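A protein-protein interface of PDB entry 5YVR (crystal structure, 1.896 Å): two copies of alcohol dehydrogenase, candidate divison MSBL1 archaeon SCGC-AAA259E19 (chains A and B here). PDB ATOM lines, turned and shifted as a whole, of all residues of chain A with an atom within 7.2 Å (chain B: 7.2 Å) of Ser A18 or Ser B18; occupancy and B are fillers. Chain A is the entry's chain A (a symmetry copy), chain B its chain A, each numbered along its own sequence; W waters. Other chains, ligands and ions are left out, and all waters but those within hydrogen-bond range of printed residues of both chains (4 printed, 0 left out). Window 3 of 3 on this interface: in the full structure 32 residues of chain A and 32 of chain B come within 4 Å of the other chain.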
ATOM      1  N   HIS A  14     -36.092  27.641 -21.448  1.00  0.00           N
ATOM      2  CA  HIS A  14     -34.845  27.924 -22.129  1.00  0.00           C
ATOM      3  C   HIS A  14     -34.794  27.023 -23.340  1.00  0.00           C
ATOM      4  O   HIS A  14     -35.019  25.812 -23.210  1.00  0.00           O
ATOM      5  CB  HIS A  14     -33.681  27.644 -21.198  1.00  0.00           C
ATOM      6  CG  HIS A  14     -32.391  27.313 -21.864  1.00  0.00           C
ATOM      7  ND1 HIS A  14     -31.266  28.101 -21.708  1.00  0.00           N
ATOM      8  CD2 HIS A  14     -31.993  26.212 -22.558  1.00  0.00           C
ATOM      9  CE1 HIS A  14     -30.248  27.535 -22.338  1.00  0.00           C
ATOM     10  NE2 HIS A  14     -30.666  26.387 -22.861  1.00  0.00           N
ATOM     11  N   ASN A  15     -34.512  27.616 -24.496  1.00  0.00           N
ATOM     12  CA  ASN A  15     -34.343  26.872 -25.750  1.00  0.00           C
ATOM     13  C   ASN A  15     -33.097  27.360 -26.460  1.00  0.00           C
ATOM     14  O   ASN A  15     -33.016  28.529 -26.830  1.00  0.00           O
ATOM     15  CB  ASN A  15     -35.562  27.021 -26.663  1.00  0.00           C
ATOM     16  CG  ASN A  15     -36.757  26.289 -26.112  1.00  0.00           C
ATOM     17  OD1 ASN A  15     -37.660  26.920 -25.568  1.00  0.00           O
ATOM     18  ND2 ASN A  15     -36.760  24.940 -26.214  1.00  0.00           N
ATOM     19  N   LEU A  16     -32.149  26.461 -26.669  1.00  0.00           N
ATOM     20  CA  LEU A  16     -30.917  26.801 -27.369  1.00  0.00           C
ATOM     21  C   LEU A  16     -30.530  25.666 -28.295  1.00  0.00           C
ATOM     22  O   LEU A  16     -30.232  24.564 -27.814  1.00  0.00           O
ATOM     23  CB  LEU A  16     -29.790  27.060 -26.365  1.00  0.00           C
ATOM     24  CG  LEU A  16     -28.439  27.501 -26.929  1.00  0.00           C
ATOM     25  CD1 LEU A  16     -28.544  28.811 -27.758  1.00  0.00           C
ATOM     26  CD2 LEU A  16     -27.445  27.623 -25.762  1.00  0.00           C
ATOM     27  N   PRO A  17     -30.511  25.897 -29.608  1.00  0.00           N
ATOM     28  CA  PRO A  17     -30.134  24.830 -30.543  1.00  0.00           C
ATOM     29  C   PRO A  17     -28.692  24.404 -30.310  1.00  0.00           C
ATOM     30  O   PRO A  17     -27.876  25.150 -29.748  1.00  0.00           O
ATOM     31  CB  PRO A  17     -30.313  25.501 -31.937  1.00  0.00           C
ATOM     32  CG  PRO A  17     -31.313  26.609 -31.707  1.00  0.00           C
ATOM     33  CD  PRO A  17     -30.859  27.156 -30.307  1.00  0.00           C
ATOM     34  N   SER A  18     -28.357  23.219 -30.808  1.00  0.00           N
ATOM     35  CA  SER A  18     -26.975  22.747 -30.762  1.00  0.00           C
ATOM     36  C   SER A  18     -26.006  23.790 -31.343  1.00  0.00           C
ATOM     37  O   SER A  18     -26.305  24.445 -32.349  1.00  0.00           O
ATOM     38  CB  SER A  18     -26.873  21.423 -31.530  1.00  0.00           C
ATOM     39  OG  SER A  18     -25.564  21.130 -31.974  1.00  0.00           O
ATOM     40  N   SER A  19     -24.854  23.968 -30.682  1.00  0.00           N
ATOM     41  CA  SER A  19     -23.853  24.950 -31.098  1.00  0.00           C
ATOM     42  C   SER A  19     -22.488  24.259 -31.142  1.00  0.00           C
ATOM     43  O   SER A  19     -22.165  23.432 -30.269  1.00  0.00           O
ATOM     44  CB  SER A  19     -23.814  26.193 -30.133  1.00  0.00           C
ATOM     45  OG  SER A  19     -23.558  25.793 -28.785  1.00  0.00           O
ATOM     46  N   ASP A  20     -21.712  24.588 -32.184  1.00  0.00           N
ATOM     47  CA  ASP A  20     -20.380  24.044 -32.453  1.00  0.00           C
ATOM     48  C   ASP A  20     -19.552  25.248 -32.917  1.00  0.00           C
ATOM     49  O   ASP A  20     -19.740  25.719 -34.045  1.00  0.00           O
ATOM     50  CB  ASP A  20     -20.431  22.934 -33.532  1.00  0.00           C
ATOM     51  CG  ASP A  20     -19.068  22.248 -33.763  1.00  0.00           C
ATOM     52  OD1 ASP A  20     -18.037  22.686 -33.197  1.00  0.00           O
ATOM     53  OD2 ASP A  20     -19.018  21.238 -34.506  1.00  0.00           O
ATOM     54  N   VAL A 165     -23.987  32.480 -34.201  1.00  0.00           N
ATOM     55  CA  VAL A 165     -24.646  31.613 -33.224  1.00  0.00           C
ATOM     56  C   VAL A 165     -26.047  32.126 -32.855  1.00  0.00           C
ATOM     57  O   VAL A 165     -26.372  32.232 -31.669  1.00  0.00           O
ATOM     58  CB  VAL A 165     -23.769  31.422 -31.945  1.00  0.00           C
ATOM     59  CG1 VAL A 165     -22.617  30.442 -32.212  1.00  0.00           C
ATOM     60  CG2 VAL A 165     -23.186  32.820 -31.375  1.00  0.00           C
ATOM     61  N   LYS A 185     -34.597  26.772 -34.747  1.00  0.00           N
ATOM     62  CA  LYS A 185     -33.539  25.778 -34.582  1.00  0.00           C
ATOM     63  C   LYS A 185     -33.050  25.246 -35.929  1.00  0.00           C
ATOM     64  O   LYS A 185     -31.859  24.929 -36.069  1.00  0.00           O
ATOM     65  CB  LYS A 185     -34.007  24.616 -33.684  1.00  0.00           C
ATOM     66  CG  LYS A 185     -35.150  23.788 -34.249  1.00  0.00           C
ATOM     67  CD  LYS A 185     -35.665  22.791 -33.217  1.00  0.00           C
ATOM     68  CE  LYS A 185     -36.815  22.018 -33.843  1.00  0.00           C
ATOM     69  NZ  LYS A 185     -37.232  20.732 -33.191  1.00  0.00           N
ATOM     70  N   PHE A 188     -30.248  27.533 -37.404  1.00  0.00           N
ATOM     71  CA  PHE A 188     -29.085  27.849 -36.578  1.00  0.00           C
ATOM     72  C   PHE A 188     -27.872  27.182 -37.209  1.00  0.00           C
ATOM     73  O   PHE A 188     -27.958  26.018 -37.590  1.00  0.00           O
ATOM     74  CB  PHE A 188     -29.304  27.344 -35.125  1.00  0.00           C
ATOM     75  CG  PHE A 188     -28.287  27.872 -34.107  1.00  0.00           C
ATOM     76  CD1 PHE A 188     -26.979  27.340 -34.034  1.00  0.00           C
ATOM     77  CD2 PHE A 188     -28.670  28.848 -33.172  1.00  0.00           C
ATOM     78  CE1 PHE A 188     -26.066  27.800 -33.007  1.00  0.00           C
ATOM     79  CE2 PHE A 188     -27.760  29.327 -32.188  1.00  0.00           C
ATOM     80  CZ  PHE A 188     -26.470  28.807 -32.139  1.00  0.00           C
ATOM     81  N   PRO A 189     -26.740  27.883 -37.364  1.00  0.00           N
ATOM     82  CA  PRO A 189     -25.629  27.299 -38.130  1.00  0.00           C
ATOM     83  C   PRO A 189     -25.144  26.004 -37.486  1.00  0.00           C
ATOM     84  O   PRO A 189     -25.058  25.875 -36.254  1.00  0.00           O
ATOM     85  CB  PRO A 189     -24.550  28.386 -38.109  1.00  0.00           C
ATOM     86  CG  PRO A 189     -25.333  29.702 -37.978  1.00  0.00           C
ATOM     87  CD  PRO A 189     -26.556  29.315 -37.095  1.00  0.00           C
ATOM     88  N   LYS A 190     -24.860  25.024 -38.344  1.00  0.00           N
ATOM     89  CA  LYS A 190     -24.349  23.753 -37.849  1.00  0.00           C
ATOM     90  C   LYS A 190     -22.966  23.905 -37.247  1.00  0.00           C
ATOM     91  O   LYS A 190     -22.632  23.219 -36.279  1.00  0.00           O
ATOM     92  CB  LYS A 190     -24.290  22.721 -38.984  1.00  0.00           C
ATOM     93  CG  LYS A 190     -25.606  22.545 -39.677  1.00  0.00           C
ATOM     94  CD  LYS A 190     -26.720  22.010 -38.759  1.00  0.00           C
ATOM     95  CE  LYS A 190     -27.896  21.592 -39.652  1.00  0.00           C
ATOM     96  NZ  LYS A 190     -29.160  21.752 -38.914  1.00  0.00           N
ATOM     97  N   VAL A 191     -22.122  24.740 -37.854  1.00  0.00           N
ATOM     98  CA  VAL A 191     -20.767  24.974 -37.365  1.00  0.00           C
ATOM     99  C   VAL A 191     -20.476  26.475 -37.507  1.00  0.00           C
ATOM    100  O   VAL A 191     -20.866  27.099 -38.503  1.00  0.00           O
ATOM    101  CB  VAL A 191     -19.712  24.171 -38.143  1.00  0.00           C
ATOM    102  CG1 VAL A 191     -18.314  24.491 -37.602  1.00  0.00           C
ATOM    103  CG2 VAL A 191     -20.015  22.650 -38.115  1.00  0.00           C
ATOM    104  N   SER A 192     -19.772  27.028 -36.525  1.00  0.00           N
ATOM    105  CA  SER A 192     -19.544  28.470 -36.422  1.00  0.00           C
ATOM    106  C   SER A 192     -18.043  28.656 -36.295  1.00  0.00           C
ATOM    107  O   SER A 192     -17.411  28.065 -35.412  1.00  0.00           O
ATOM    108  CB  SER A 192     -20.274  29.081 -35.198  1.00  0.00           C
ATOM    109  OG  SER A 192     -21.663  28.767 -35.199  1.00  0.00           O
ATOM    110  N   HIS B  14     -16.048  24.984 -28.761  1.00  0.00           N
ATOM    111  CA  HIS B  14     -17.198  24.894 -27.884  1.00  0.00           C
ATOM    112  C   HIS B  14     -18.175  23.948 -28.541  1.00  0.00           C
ATOM    113  O   HIS B  14     -18.476  24.110 -29.731  1.00  0.00           O
ATOM    114  CB  HIS B  14     -17.813  26.269 -27.709  1.00  0.00           C
ATOM    115  CG  HIS B  14     -19.261  26.286 -27.361  1.00  0.00           C
ATOM    116  ND1 HIS B  14     -19.720  26.825 -26.174  1.00  0.00           N
ATOM    117  CD2 HIS B  14     -20.366  25.977 -28.092  1.00  0.00           C
ATOM    118  CE1 HIS B  14     -21.043  26.783 -26.160  1.00  0.00           C
ATOM    119  NE2 HIS B  14     -21.457  26.272 -27.315  1.00  0.00           N
ATOM    120  N   ASN B  15     -18.649  22.973 -27.771  1.00  0.00           N
ATOM    121  CA  ASN B  15     -19.668  22.021 -28.231  1.00  0.00           C
ATOM    122  C   ASN B  15     -20.739  21.881 -27.170  1.00  0.00           C
ATOM    123  O   ASN B  15     -20.452  21.447 -26.057  1.00  0.00           O
ATOM    124  CB  ASN B  15     -19.060  20.654 -28.550  1.00  0.00           C
ATOM    125  CG  ASN B  15     -18.206  20.705 -29.789  1.00  0.00           C
ATOM    126  OD1 ASN B  15     -16.982  20.714 -29.685  1.00  0.00           O
ATOM    127  ND2 ASN B  15     -18.844  20.775 -30.980  1.00  0.00           N
ATOM    128  N   LEU B  16     -21.967  22.222 -27.525  1.00  0.00           N
ATOM    129  CA  LEU B  16     -23.090  22.102 -26.603  1.00  0.00           C
ATOM    130  C   LEU B  16     -24.304  21.585 -27.346  1.00  0.00           C
ATOM    131  O   LEU B  16     -24.808  22.277 -28.242  1.00  0.00           O
ATOM    132  CB  LEU B  16     -23.405  23.461 -25.971  1.00  0.00           C
ATOM    133  CG  LEU B  16     -24.514  23.502 -24.920  1.00  0.00           C
ATOM    134  CD1 LEU B  16     -24.224  22.560 -23.718  1.00  0.00           C
ATOM    135  CD2 LEU B  16     -24.714  24.963 -24.486  1.00  0.00           C
ATOM    136  N   PRO B  17     -24.803  20.398 -27.000  1.00  0.00           N
ATOM    137  CA  PRO B  17     -25.983  19.861 -27.686  1.00  0.00           C
ATOM    138  C   PRO B  17     -27.191  20.755 -27.445  1.00  0.00           C
ATOM    139  O   PRO B  17     -27.247  21.525 -26.475  1.00  0.00           O
ATOM    140  CB  PRO B  17     -26.170  18.462 -27.028  1.00  0.00           C
ATOM    141  CG  PRO B  17     -24.800  18.092 -26.513  1.00  0.00           C
ATOM    142  CD  PRO B  17     -24.288  19.472 -25.964  1.00  0.00           C
ATOM    143  N   SER B  18     -28.197  20.603 -28.299  1.00  0.00           N
ATOM    144  CA  SER B  18     -29.461  21.311 -28.108  1.00  0.00           C
ATOM    145  C   SER B  18     -30.014  21.095 -26.690  1.00  0.00           C
ATOM    146  O   SER B  18     -29.941  19.990 -26.139  1.00  0.00           O
ATOM    147  CB  SER B  18     -30.467  20.832 -29.162  1.00  0.00           C
ATOM    148  OG  SER B  18     -31.813  21.049 -28.795  1.00  0.00           O
ATOM    149  N   SER B  19     -30.539  22.171 -26.084  1.00  0.00           N
ATOM    150  CA  SER B  19     -31.070  22.124 -24.723  1.00  0.00           C
ATOM    151  C   SER B  19     -32.457  22.770 -24.725  1.00  0.00           C
ATOM    152  O   SER B  19     -32.685  23.788 -25.404  1.00  0.00           O
ATOM    153  CB  SER B  19     -30.122  22.849 -23.697  1.00  0.00           C
ATOM    154  OG  SER B  19     -29.896  24.210 -24.075  1.00  0.00           O
ATOM    155  N   ASP B  20     -33.382  22.146 -23.980  1.00  0.00           N
ATOM    156  CA  ASP B  20     -34.779  22.559 -23.843  1.00  0.00           C
ATOM    157  C   ASP B  20     -35.100  22.367 -22.356  1.00  0.00           C
ATOM    158  O   ASP B  20     -35.248  21.224 -21.907  1.00  0.00           O
ATOM    159  CB  ASP B  20     -35.710  21.711 -24.743  1.00  0.00           C
ATOM    160  CG  ASP B  20     -37.177  22.190 -24.723  1.00  0.00           C
ATOM    161  OD1 ASP B  20     -37.535  23.095 -23.931  1.00  0.00           O
ATOM    162  OD2 ASP B  20     -37.993  21.672 -25.524  1.00  0.00           O
ATOM    163  N   VAL B 165     -29.028  18.400 -17.772  1.00  0.00           N
ATOM    164  CA  VAL B 165     -28.462  19.082 -18.936  1.00  0.00           C
ATOM    165  C   VAL B 165     -26.979  18.731 -19.141  1.00  0.00           C
ATOM    166  O   VAL B 165     -26.151  19.629 -19.312  1.00  0.00           O
ATOM    167  CB  VAL B 165     -28.659  20.630 -18.843  1.00  0.00           C
ATOM    168  CG1 VAL B 165     -30.107  21.018 -19.174  1.00  0.00           C
ATOM    169  CG2 VAL B 165     -28.241  21.225 -17.398  1.00  0.00           C
ATOM    170  N   LYS B 185     -23.526  13.920 -27.525  1.00  0.00           N
ATOM    171  CA  LYS B 185     -24.715  14.653 -27.954  1.00  0.00           C
ATOM    172  C   LYS B 185     -25.931  13.735 -28.073  1.00  0.00           C
ATOM    173  O   LYS B 185     -27.061  14.174 -27.810  1.00  0.00           O
ATOM    174  CB  LYS B 185     -24.463  15.385 -29.287  1.00  0.00           C
ATOM    175  CG  LYS B 185     -24.190  14.478 -30.476  1.00  0.00           C
ATOM    176  CD  LYS B 185     -23.768  15.288 -31.696  1.00  0.00           C
ATOM    177  CE  LYS B 185     -23.493  14.317 -32.834  1.00  0.00           C
ATOM    178  NZ  LYS B 185     -23.444  14.868 -34.229  1.00  0.00           N
ATOM    179  N   PHE B 188     -27.762  13.383 -24.641  1.00  0.00           N
ATOM    180  CA  PHE B 188     -28.160  14.594 -23.924  1.00  0.00           C
ATOM    181  C   PHE B 188     -29.681  14.648 -23.912  1.00  0.00           C
ATOM    182  O   PHE B 188     -30.297  14.411 -24.947  1.00  0.00           O
ATOM    183  CB  PHE B 188     -27.565  15.850 -24.618  1.00  0.00           C
ATOM    184  CG  PHE B 188     -27.670  17.141 -23.798  1.00  0.00           C
ATOM    185  CD1 PHE B 188     -28.890  17.847 -23.695  1.00  0.00           C
ATOM    186  CD2 PHE B 188     -26.524  17.686 -23.195  1.00  0.00           C
ATOM    187  CE1 PHE B 188     -28.941  19.107 -22.982  1.00  0.00           C
ATOM    188  CE2 PHE B 188     -26.582  18.905 -22.463  1.00  0.00           C
ATOM    189  CZ  PHE B 188     -27.795  19.580 -22.354  1.00  0.00           C
ATOM    190  N   PRO B 189     -30.322  14.925 -22.770  1.00  0.00           N
ATOM    191  CA  PRO B 189     -31.787  14.804 -22.715  1.00  0.00           C
ATOM    192  C   PRO B 189     -32.449  15.746 -23.716  1.00  0.00           C
ATOM    193  O   PRO B 189     -32.023  16.896 -23.917  1.00  0.00           O
ATOM    194  CB  PRO B 189     -32.138  15.168 -21.270  1.00  0.00           C
ATOM    195  CG  PRO B 189     -30.889  14.781 -20.462  1.00  0.00           C
ATOM    196  CD  PRO B 189     -29.714  15.074 -21.440  1.00  0.00           C
ATOM    197  N   LYS B 190     -33.485  15.226 -24.374  1.00  0.00           N
ATOM    198  CA  LYS B 190     -34.223  16.045 -25.327  1.00  0.00           C
ATOM    199  C   LYS B 190     -34.964  17.172 -24.636  1.00  0.00           C
ATOM    200  O   LYS B 190     -35.095  18.263 -25.194  1.00  0.00           O
ATOM    201  CB  LYS B 190     -35.230  15.186 -26.104  1.00  0.00           C
ATOM    202  CG  LYS B 190     -34.592  14.010 -26.777  1.00  0.00           C
ATOM    203  CD  LYS B 190     -33.551  14.399 -27.842  1.00  0.00           C
ATOM    204  CE  LYS B 190     -33.217  13.136 -28.648  1.00  0.00           C
ATOM    205  NZ  LYS B 190     -31.833  13.216 -29.144  1.00  0.00           N
ATOM    206  N   VAL B 191     -35.523  16.904 -23.455  1.00  0.00           N
ATOM    207  CA  VAL B 191     -36.257  17.909 -22.692  1.00  0.00           C
ATOM    208  C   VAL B 191     -35.885  17.730 -21.214  1.00  0.00           C
ATOM    209  O   VAL B 191     -35.751  16.598 -20.732  1.00  0.00           O
ATOM    210  CB  VAL B 191     -37.781  17.778 -22.857  1.00  0.00           C
ATOM    211  CG1 VAL B 191     -38.487  18.838 -22.004  1.00  0.00           C
ATOM    212  CG2 VAL B 191     -38.203  17.852 -24.348  1.00  0.00           C
ATOM    213  N   SER B 192     -35.752  18.848 -20.507  1.00  0.00           N
ATOM    214  CA  SER B 192     -35.248  18.867 -19.133  1.00  0.00           C
ATOM    215  C   SER B 192     -36.278  19.620 -18.311  1.00  0.00           C
ATOM    216  O   SER B 192     -36.636  20.754 -18.644  1.00  0.00           O
ATOM    217  CB  SER B 192     -33.864  19.560 -19.038  1.00  0.00           C
ATOM    218  OG  SER B 192     -32.921  18.984 -19.938  1.00  0.00           O
HETATM  219  O   HOH W   1     -21.786  20.754 -30.824  1.00  0.00           O
HETATM  220  O   HOH W   2     -25.939  24.997 -27.843  1.00  0.00           O
HETATM  221  O   HOH W   3     -27.973  24.093 -25.940  1.00  0.00           O
HETATM  222  O   HOH W   4     -34.408  23.784 -27.561  1.00  0.00           O
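Hydrophobic or aromatic side chains of chain A that line the printed part of chain B: His A14 and Leu A16.
Among the printed residues, 15 pairs touch across the chains.
Among the printed residues, no Asp or Glu carboxylate lies within 4 Å of a Lys or Arg side-chain nitrogen of the other chain.
The backbone carbonyl oxygen (O) of Asp B20 is in hydrogen-bond range of the backbone NH (N) of Ser B192 (2.8 Å).
The backbone carbonyl oxygen (O) of Asp A20 is in hydrogen-bond range of the backbone NH (N) of Ser A192 (2.8 Å).
A ring nitrogen (NE2) of His B14 sits at hydrogen-bond distance from the side-chain hydroxyl (OG) of Ser A19 (2.6 Å).
ND2 of Asn B15 sits at hydrogen-bond distance from OD1 of Asp A20 (3.0 Å).
The backbone carbonyl oxygen of Leu B16 sits at hydrogen-bond distance from the backbone NH of Ser A19 (3.0 Å).
The side-chain hydroxyl (OG) of Ser B19 sits at hydrogen-bond distance from a ring nitrogen (NE2) of His A14, at 2.6 Å.
The backbone carbonyl oxygen of Leu A16 lies within hydrogen-bond range of the backbone NH of Ser B19 (3.0 Å).
The side-chain carboxylate of Asp B20 lies within hydrogen-bond range of the side-chain amide nitrogen of Asn A15, 3.0 Å away.
Asn A15 touches Ser B19, and with the chains exchanged Ser A19 touches Asn B15.
Leu A16 touches Ser B19, and with the chains exchanged Ser A19 touches Leu B16.
Pro A17 touches Ser B18, and with the chains exchanged Ser A18 touches Pro B17.
Ser A18 touches its own counterpart, Ser B18.
14 positions are printed for both chains.
Of the 15 pairs that touch across the chains among the printed residues, 15 have their exchanged pair printed and touching as well.
Ser A18 touches just these residues of chain B: Leu B16 (3.4 Å), Pro B17 (3.9 Å) and Ser B18 (3.5 Å).
Printed residues of chain B within 4 Å of Leu A16: Ser B18 (3.4 Å) and Ser B19 (3.0 Å).
Of the printed residues of chain B, Pro A17 touches Ser B18.
Printed residues of chain A within 4 Å of Leu B16: Ser A18 and Ser A19.
Printed residues of chain B within 4 Å of Asn A15: Ser B19 and Asp B20.
Of the printed residues of chain A, Pro B17 touches Ser A18 (3.9 Å).
Val B191 touches none of the printed residues of chain A.
The nearest printed residue of chain B that does not touch Asn A15 is Ser B18 (6.8 Å).
Water W3 lies within hydrogen-bond range of OG of Ser B19, O of Pro B17 and O of Leu A16.
Water W2 lies within hydrogen-bond range of OG of Ser A19 (2.7 Å), O of Pro A17 (2.7 Å) and O of Leu B16 (3.0 Å).
Water W4 lies within hydrogen-bond range of the backbone carbonyl oxygen (O) of Ser B19 (2.8 Å) and the side-chain amide nitrogen (ND2) of Asn A15 (2.9 Å).
Water W1 lies within hydrogen-bond range of the backbone carbonyl oxygen (O) of Ser A19 (2.8 Å) and the side-chain amide nitrogen (ND2) of Asn B15 (2.9 Å).
Among the printed residues, pairs that only touch across the chains: Asp A20 with His B14 (3.3 Å), His A14 with Asp B20 (3.3 Å), Leu A16 with Ser B18 (3.4 Å), Ser A18 with Leu B16 (3.4 Å), Ser A18 with Ser B18 (3.5 Å), Ser A19 with Asn B15 (3.5 Å), Asn A15 with Ser B19 (3.5 Å), Pro A17 with Ser B18 (3.9 Å) and Ser A18 with Pro B17 (3.9 Å).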
